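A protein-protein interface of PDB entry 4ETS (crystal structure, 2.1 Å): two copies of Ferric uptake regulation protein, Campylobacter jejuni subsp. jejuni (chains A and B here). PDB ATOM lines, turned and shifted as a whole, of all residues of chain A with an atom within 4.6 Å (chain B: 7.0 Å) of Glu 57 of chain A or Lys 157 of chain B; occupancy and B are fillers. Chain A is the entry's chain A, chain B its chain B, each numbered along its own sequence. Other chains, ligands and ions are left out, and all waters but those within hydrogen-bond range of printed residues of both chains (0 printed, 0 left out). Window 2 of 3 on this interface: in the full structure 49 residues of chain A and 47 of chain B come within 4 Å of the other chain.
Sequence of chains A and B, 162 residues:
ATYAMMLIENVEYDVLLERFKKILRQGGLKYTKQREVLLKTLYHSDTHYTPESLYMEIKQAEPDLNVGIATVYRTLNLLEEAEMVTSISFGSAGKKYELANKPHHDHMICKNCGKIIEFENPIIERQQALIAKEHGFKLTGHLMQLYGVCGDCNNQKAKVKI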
ATOM      1  N   THR A  41      31.439  -5.389   1.704  1.00  0.00           N
ATOM      2  CA  THR A  41      30.308  -6.200   2.183  1.00  0.00           C
ATOM      3  C   THR A  41      30.651  -6.807   3.554  1.00  0.00           C
ATOM      4  O   THR A  41      29.771  -6.923   4.426  1.00  0.00           O
ATOM      5  CB  THR A  41      29.898  -7.348   1.219  1.00  0.00           C
ATOM      6  OG1 THR A  41      29.690  -6.827  -0.085  1.00  0.00           O
ATOM      7  CG2 THR A  41      28.573  -7.984   1.700  1.00  0.00           C
ATOM      8  N   HIS A  44      30.909  -3.352   6.168  1.00  0.00           N
ATOM      9  CA  HIS A  44      29.636  -2.699   6.520  1.00  0.00           C
ATOM     10  C   HIS A  44      28.640  -3.629   7.218  1.00  0.00           C
ATOM     11  O   HIS A  44      27.576  -3.173   7.632  1.00  0.00           O
ATOM     12  CB  HIS A  44      28.998  -1.912   5.334  1.00  0.00           C
ATOM     13  CG  HIS A  44      29.844  -0.759   4.838  1.00  0.00           C
ATOM     14  ND1 HIS A  44      30.225   0.298   5.643  1.00  0.00           N
ATOM     15  CD2 HIS A  44      30.399  -0.510   3.622  1.00  0.00           C
ATOM     16  CE1 HIS A  44      30.991   1.133   4.959  1.00  0.00           C
ATOM     17  NE2 HIS A  44      31.091   0.677   3.723  1.00  0.00           N
ATOM     18  N   SER A  45      28.944  -4.917   7.378  1.00  0.00           N
ATOM     19  CA  SER A  45      27.909  -5.781   7.990  1.00  0.00           C
ATOM     20  C   SER A  45      28.340  -6.298   9.310  1.00  0.00           C
ATOM     21  O   SER A  45      29.530  -6.315   9.611  1.00  0.00           O
ATOM     22  CB  SER A  45      27.494  -6.980   7.100  1.00  0.00           C
ATOM     23  OG  SER A  45      28.626  -7.719   6.708  1.00  0.00           O
ATOM     24  N   THR A  47      27.189  -9.450  10.440  1.00  0.00           N
ATOM     25  CA  THR A  47      26.923 -10.907  10.495  1.00  0.00           C
ATOM     26  C   THR A  47      28.119 -11.677   9.995  1.00  0.00           C
ATOM     27  O   THR A  47      28.983 -11.086   9.333  1.00  0.00           O
ATOM     28  CB  THR A  47      25.705 -11.309   9.647  1.00  0.00           C
ATOM     29  OG1 THR A  47      25.852 -10.845   8.287  1.00  0.00           O
ATOM     30  CG2 THR A  47      24.374 -10.762  10.268  1.00  0.00           C
ATOM     31  N   TYR A  49      29.806 -14.776   7.615  1.00  0.00           N
ATOM     32  CA  TYR A  49      29.507 -15.361   6.289  1.00  0.00           C
ATOM     33  C   TYR A  49      30.228 -16.657   6.077  1.00  0.00           C
ATOM     34  O   TYR A  49      31.328 -16.838   6.600  1.00  0.00           O
ATOM     35  CB  TYR A  49      29.925 -14.420   5.174  1.00  0.00           C
ATOM     36  CG  TYR A  49      29.087 -13.179   5.057  1.00  0.00           C
ATOM     37  CD1 TYR A  49      29.497 -11.976   5.653  1.00  0.00           C
ATOM     38  CD2 TYR A  49      27.901 -13.194   4.332  1.00  0.00           C
ATOM     39  CE1 TYR A  49      28.712 -10.804   5.506  1.00  0.00           C
ATOM     40  CE2 TYR A  49      27.112 -12.069   4.182  1.00  0.00           C
ATOM     41  CZ  TYR A  49      27.532 -10.869   4.794  1.00  0.00           C
ATOM     42  OH  TYR A  49      26.769  -9.761   4.640  1.00  0.00           O
ATOM     43  N   SER A  53      27.355 -17.923   1.466  1.00  0.00           N
ATOM     44  CA  SER A  53      26.476 -16.803   1.729  1.00  0.00           C
ATOM     45  C   SER A  53      27.065 -15.471   1.291  1.00  0.00           C
ATOM     46  O   SER A  53      26.339 -14.556   0.877  1.00  0.00           O
ATOM     47  CB  SER A  53      26.104 -16.688   3.187  1.00  0.00           C
ATOM     48  OG  SER A  53      25.415 -15.461   3.293  1.00  0.00           O
ATOM     49  N   LEU A  54      28.385 -15.349   1.385  1.00  0.00           N
ATOM     50  CA  LEU A  54      28.989 -14.066   0.999  1.00  0.00           C
ATOM     51  C   LEU A  54      28.832 -13.903  -0.528  1.00  0.00           C
ATOM     52  O   LEU A  54      28.504 -12.816  -1.043  1.00  0.00           O
ATOM     53  CB  LEU A  54      30.463 -13.997   1.430  1.00  0.00           C
ATOM     54  CG  LEU A  54      31.209 -12.664   1.183  1.00  0.00           C
ATOM     55  CD1 LEU A  54      30.418 -11.485   1.683  1.00  0.00           C
ATOM     56  CD2 LEU A  54      32.615 -12.634   1.830  1.00  0.00           C
ATOM     57  N   TYR A  55      29.097 -14.996  -1.246  1.00  0.00           N
ATOM     58  CA  TYR A  55      28.892 -15.014  -2.713  1.00  0.00           C
ATOM     59  C   TYR A  55      27.452 -14.614  -3.100  1.00  0.00           C
ATOM     60  O   TYR A  55      27.272 -13.808  -3.996  1.00  0.00           O
ATOM     61  CB  TYR A  55      29.303 -16.388  -3.283  1.00  0.00           C
ATOM     62  CG  TYR A  55      28.599 -16.809  -4.539  1.00  0.00           C
ATOM     63  CD1 TYR A  55      28.934 -16.253  -5.792  1.00  0.00           C
ATOM     64  CD2 TYR A  55      27.607 -17.816  -4.483  1.00  0.00           C
ATOM     65  CE1 TYR A  55      28.271 -16.703  -6.977  1.00  0.00           C
ATOM     66  CE2 TYR A  55      26.946 -18.260  -5.643  1.00  0.00           C
ATOM     67  CZ  TYR A  55      27.266 -17.677  -6.870  1.00  0.00           C
ATOM     68  OH  TYR A  55      26.616 -18.127  -7.977  1.00  0.00           O
ATOM     69  N   MET A  56      26.447 -15.149  -2.395  1.00  0.00           N
ATOM     70  CA  MET A  56      25.025 -14.860  -2.688  1.00  0.00           C
ATOM     71  C   MET A  56      24.701 -13.434  -2.432  1.00  0.00           C
ATOM     72  O   MET A  56      24.081 -12.766  -3.287  1.00  0.00           O
ATOM     73  CB  MET A  56      24.081 -15.741  -1.855  1.00  0.00           C
ATOM     74  CG  MET A  56      24.184 -17.230  -2.212  1.00  0.00           C
ATOM     75  SD  MET A  56      23.256 -17.734  -3.699  1.00  0.00           S
ATOM     76  CE  MET A  56      23.836 -16.699  -5.014  1.00  0.00           C
ATOM     77  N   GLU A  57      25.132 -12.930  -1.265  1.00  0.00           N
ATOM     78  CA  GLU A  57      24.883 -11.518  -0.971  1.00  0.00           C
ATOM     79  C   GLU A  57      25.456 -10.621  -2.037  1.00  0.00           C
ATOM     80  O   GLU A  57      24.793  -9.666  -2.477  1.00  0.00           O
ATOM     81  CB  GLU A  57      25.438 -11.101   0.401  1.00  0.00           C
ATOM     82  CG  GLU A  57      25.227  -9.598   0.643  1.00  0.00           C
ATOM     83  CD  GLU A  57      23.733  -9.201   0.556  1.00  0.00           C
ATOM     84  OE1 GLU A  57      23.029  -9.397   1.564  1.00  0.00           O
ATOM     85  OE2 GLU A  57      23.257  -8.683  -0.496  1.00  0.00           O
ATOM     86  N   ILE A  58      26.696 -10.899  -2.467  1.00  0.00           N
ATOM     87  CA  ILE A  58      27.351 -10.065  -3.505  1.00  0.00           C
ATOM     88  C   ILE A  58      26.635 -10.172  -4.874  1.00  0.00           C
ATOM     89  O   ILE A  58      26.454  -9.171  -5.616  1.00  0.00           O
ATOM     90  CB  ILE A  58      28.840 -10.457  -3.669  1.00  0.00           C
ATOM     91  CG1 ILE A  58      29.664 -10.042  -2.450  1.00  0.00           C
ATOM     92  CG2 ILE A  58      29.422  -9.887  -4.939  1.00  0.00           C
ATOM     93  CD1 ILE A  58      31.106 -10.631  -2.456  1.00  0.00           C
ATOM     94  N   LYS A  59      26.250 -11.394  -5.197  1.00  0.00           N
ATOM     95  CA  LYS A  59      25.599 -11.711  -6.465  1.00  0.00           C
ATOM     96  C   LYS A  59      24.263 -10.982  -6.454  1.00  0.00           C
ATOM     97  O   LYS A  59      23.947 -10.217  -7.396  1.00  0.00           O
ATOM     98  CB  LYS A  59      25.443 -13.257  -6.587  1.00  0.00           C
ATOM     99  CG  LYS A  59      24.739 -13.819  -7.849  1.00  0.00           C
ATOM    100  CD  LYS A  59      25.563 -13.648  -9.147  1.00  0.00           C
ATOM    101  CE  LYS A  59      25.209 -12.340  -9.909  1.00  0.00           C
ATOM    102  NZ  LYS A  59      26.009 -12.134 -11.167  1.00  0.00           N
ATOM    103  N   GLN A  60      23.522 -11.155  -5.351  1.00  0.00           N
ATOM    104  CA  GLN A  60      22.218 -10.460  -5.157  1.00  0.00           C
ATOM    105  C   GLN A  60      22.356  -8.907  -5.242  1.00  0.00           C
ATOM    106  O   GLN A  60      21.624  -8.256  -5.995  1.00  0.00           O
ATOM    107  CB  GLN A  60      21.507 -10.952  -3.861  1.00  0.00           C
ATOM    108  CG  GLN A  60      20.345 -10.050  -3.348  1.00  0.00           C
ATOM    109  CD  GLN A  60      19.842 -10.497  -1.960  1.00  0.00           C
ATOM    110  OE1 GLN A  60      20.391 -11.426  -1.363  1.00  0.00           O
ATOM    111  NE2 GLN A  60      18.802  -9.832  -1.447  1.00  0.00           N
ATOM    112  N   ALA A  61      23.344  -8.322  -4.565  1.00  0.00           N
ATOM    113  CA  ALA A  61      23.433  -6.849  -4.508  1.00  0.00           C
ATOM    114  C   ALA A  61      24.046  -6.171  -5.709  1.00  0.00           C
ATOM    115  O   ALA A  61      23.735  -5.003  -5.966  1.00  0.00           O
ATOM    116  CB  ALA A  61      24.157  -6.380  -3.249  1.00  0.00           C
ATOM    117  N   ASN B 112      27.471   0.434   9.569  1.00  0.00           N
ATOM    118  CA  ASN B 112      26.330  -0.011   8.714  1.00  0.00           C
ATOM    119  C   ASN B 112      25.561   1.171   8.075  1.00  0.00           C
ATOM    120  O   ASN B 112      25.833   1.544   6.883  1.00  0.00           O
ATOM    121  CB  ASN B 112      25.389  -1.017   9.420  1.00  0.00           C
ATOM    122  CG  ASN B 112      24.490  -1.694   8.411  1.00  0.00           C
ATOM    123  OD1 ASN B 112      24.238  -1.088   7.370  1.00  0.00           O
ATOM    124  ND2 ASN B 112      24.019  -2.911   8.673  1.00  0.00           N
ATOM    125  N   CYS B 153      21.367  -1.318  13.862  1.00  0.00           N
ATOM    126  CA  CYS B 153      22.064  -2.116  12.883  1.00  0.00           C
ATOM    127  C   CYS B 153      22.626  -3.453  13.374  1.00  0.00           C
ATOM    128  O   CYS B 153      23.424  -4.131  12.642  1.00  0.00           O
ATOM    129  CB  CYS B 153      23.151  -1.271  12.230  1.00  0.00           C
ATOM    130  SG  CYS B 153      22.397   0.118  11.434  1.00  0.00           S
ATOM    131  N   ASN B 154      22.234  -3.812  14.605  1.00  0.00           N
ATOM    132  CA  ASN B 154      22.637  -5.094  15.195  1.00  0.00           C
ATOM    133  C   ASN B 154      22.383  -6.324  14.320  1.00  0.00           C
ATOM    134  O   ASN B 154      21.262  -6.531  13.854  1.00  0.00           O
ATOM    135  CB  ASN B 154      21.987  -5.312  16.575  1.00  0.00           C
ATOM    136  CG  ASN B 154      22.797  -4.686  17.684  1.00  0.00           C
ATOM    137  OD1 ASN B 154      23.689  -5.330  18.245  1.00  0.00           O
ATOM    138  ND2 ASN B 154      22.526  -3.399  17.979  1.00  0.00           N
ATOM    139  N   ASN B 155      23.450  -7.111  14.124  1.00  0.00           N
ATOM    140  CA  ASN B 155      23.415  -8.395  13.437  1.00  0.00           C
ATOM    141  C   ASN B 155      22.690  -8.277  12.101  1.00  0.00           C
ATOM    142  O   ASN B 155      21.838  -9.105  11.769  1.00  0.00           O
ATOM    143  CB  ASN B 155      22.781  -9.496  14.319  1.00  0.00           C
ATOM    144  CG  ASN B 155      23.298  -9.478  15.745  1.00  0.00           C
ATOM    145  OD1 ASN B 155      24.513  -9.407  15.988  1.00  0.00           O
ATOM    146  ND2 ASN B 155      22.373  -9.559  16.707  1.00  0.00           N
ATOM    147  N   GLN B 156      23.041  -7.236  11.345  1.00  0.00           N
ATOM    148  CA  GLN B 156      22.512  -7.055  10.022  1.00  0.00           C
ATOM    149  C   GLN B 156      23.639  -6.896   8.996  1.00  0.00           C
ATOM    150  O   GLN B 156      24.753  -6.513   9.339  1.00  0.00           O
ATOM    151  CB  GLN B 156      21.573  -5.841   9.981  1.00  0.00           C
ATOM    152  CG  GLN B 156      20.233  -6.065  10.678  1.00  0.00           C
ATOM    153  CD  GLN B 156      19.648  -4.762  11.178  1.00  0.00           C
ATOM    154  OE1 GLN B 156      19.110  -3.974  10.395  1.00  0.00           O
ATOM    155  NE2 GLN B 156      19.769  -4.516  12.491  1.00  0.00           N
ATOM    156  N   LYS B 157      23.298  -7.224   7.754  1.00  0.00           N
ATOM    157  CA  LYS B 157      24.076  -6.973   6.552  1.00  0.00           C
ATOM    158  C   LYS B 157      24.124  -5.490   6.228  1.00  0.00           C
ATOM    159  O   LYS B 157      23.284  -4.705   6.737  1.00  0.00           O
ATOM    160  CB  LYS B 157      23.375  -7.634   5.340  1.00  0.00           C
ATOM    161  CG  LYS B 157      23.321  -9.158   5.343  1.00  0.00           C
ATOM    162  CD  LYS B 157      22.283  -9.652   4.303  1.00  0.00           C
ATOM    163  CE  LYS B 157      21.002 -10.156   4.964  1.00  0.00           C
ATOM    164  NZ  LYS B 157      21.184 -11.526   5.515  1.00  0.00           N
ATOM    165  N   ALA B 158      25.056  -5.138   5.331  1.00  0.00           N
ATOM    166  CA  ALA B 158      25.112  -3.831   4.675  1.00  0.00           C
ATOM    167  C   ALA B 158      23.697  -3.371   4.294  1.00  0.00           C
ATOM    168  O   ALA B 158      22.972  -4.103   3.615  1.00  0.00           O
ATOM    169  CB  ALA B 158      26.017  -3.884   3.432  1.00  0.00           C
ATOM    170  N   LYS B 159      23.292  -2.185   4.764  1.00  0.00           N
ATOM    171  CA  LYS B 159      21.916  -1.729   4.579  1.00  0.00           C
ATOM    172  C   LYS B 159      21.650  -1.018   3.232  1.00  0.00           C
ATOM    173  O   LYS B 159      22.179   0.058   2.955  1.00  0.00           O
ATOM    174  CB  LYS B 159      21.453  -0.888   5.759  1.00  0.00           C
ATOM    175  CG  LYS B 159      20.735  -1.695   6.815  1.00  0.00           C
ATOM    176  CD  LYS B 159      20.282  -0.787   7.944  1.00  0.00           C
ATOM    177  CE  LYS B 159      19.694  -1.629   9.047  1.00  0.00           C
ATOM    178  NZ  LYS B 159      19.661  -0.887  10.357  1.00  0.00           N
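Of the 8 printed residues of chain B, 5 touch a printed residue of chain A. Along chain A the printed residues that touch a printed residue of chain B span positions 44 to 57. Among the printed residues, no Asp or Glu carboxylate lies within 4 Å of a Lys or Arg side-chain nitrogen of the other chain.
Ser 53 of chain A touches none of the printed residues of chain B. Of the printed residues of chain A, Asn 155 of chain B touches Thr 47. Of the printed residues of chain A, Gln 156 of chain B touches Ser 45 (3.5 Å) and Thr 47 (3.9 Å). Lys 157 of chain B touches just these residues of chain A: Ser 45 (3.5 Å), Tyr 49 (3.6 Å) and Glu 57 (2.9 Å). Lys 159 of chain B touches none of the printed residues of chain A. The nearest residue of chain A that does not touch Lys 157 of chain B is Thr 47 of chain A (4.2 Å).
No position is printed for both chains. Of the 9 pairs that touch across the chains among the printed residues, none has its exchanged pair printed and touching as well.
His 44 of chain A touches Asn 112 of chain B. His 44 of chain A touches Ala 158 of chain B (O to CA, 3.9 Å). CA of Ser 45 of chain A touches O of Gln 156 of chain B (3.5 Å). Ser 45 of chain A touches Lys 157 of chain B. Ser 45 of chain A touches Ala 158 of chain B. CG2 of Thr 47 of chain A touches O of Asn 155 of chain B (3.4 Å). CG2 of Thr 47 of chain A touches N of Gln 156 of chain B, at 3.9 Å. Tyr 49 of chain A touches Lys 157 of chain B. Lys 157 of chain B touches Glu 57 of chain A.
The side-chain hydroxyl (OG) of Ser 45 of chain A is in hydrogen-bond range of the backbone carbonyl oxygen (O) of Thr 41 of chain A, 2.7 Å away. The side-chain amide nitrogen (ND2) of Asn 112 of chain B sits at hydrogen-bond distance from the backbone carbonyl oxygen (O) of Lys 157 of chain B (2.7 Å). The side-chain amide oxygen (OD1) of Asn 112 of chain B is in hydrogen-bond range of the backbone NH (N) of Lys 159 of chain B, at 3.0 Å. The side-chain hydroxyl of Tyr 49 of chain A lies close to the side-chain hydroxyl of Ser 45 of chain A, 3.4 Å away. The backbone carbonyl oxygen (O) of Asn 154 of chain B sits at hydrogen-bond distance from the side-chain amide nitrogen (NE2) of Gln 156 of chain B (2.9 Å). NZ of Lys 159 of chain B lies close to OE1 of Gln 156 of chain B (3.1 Å).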
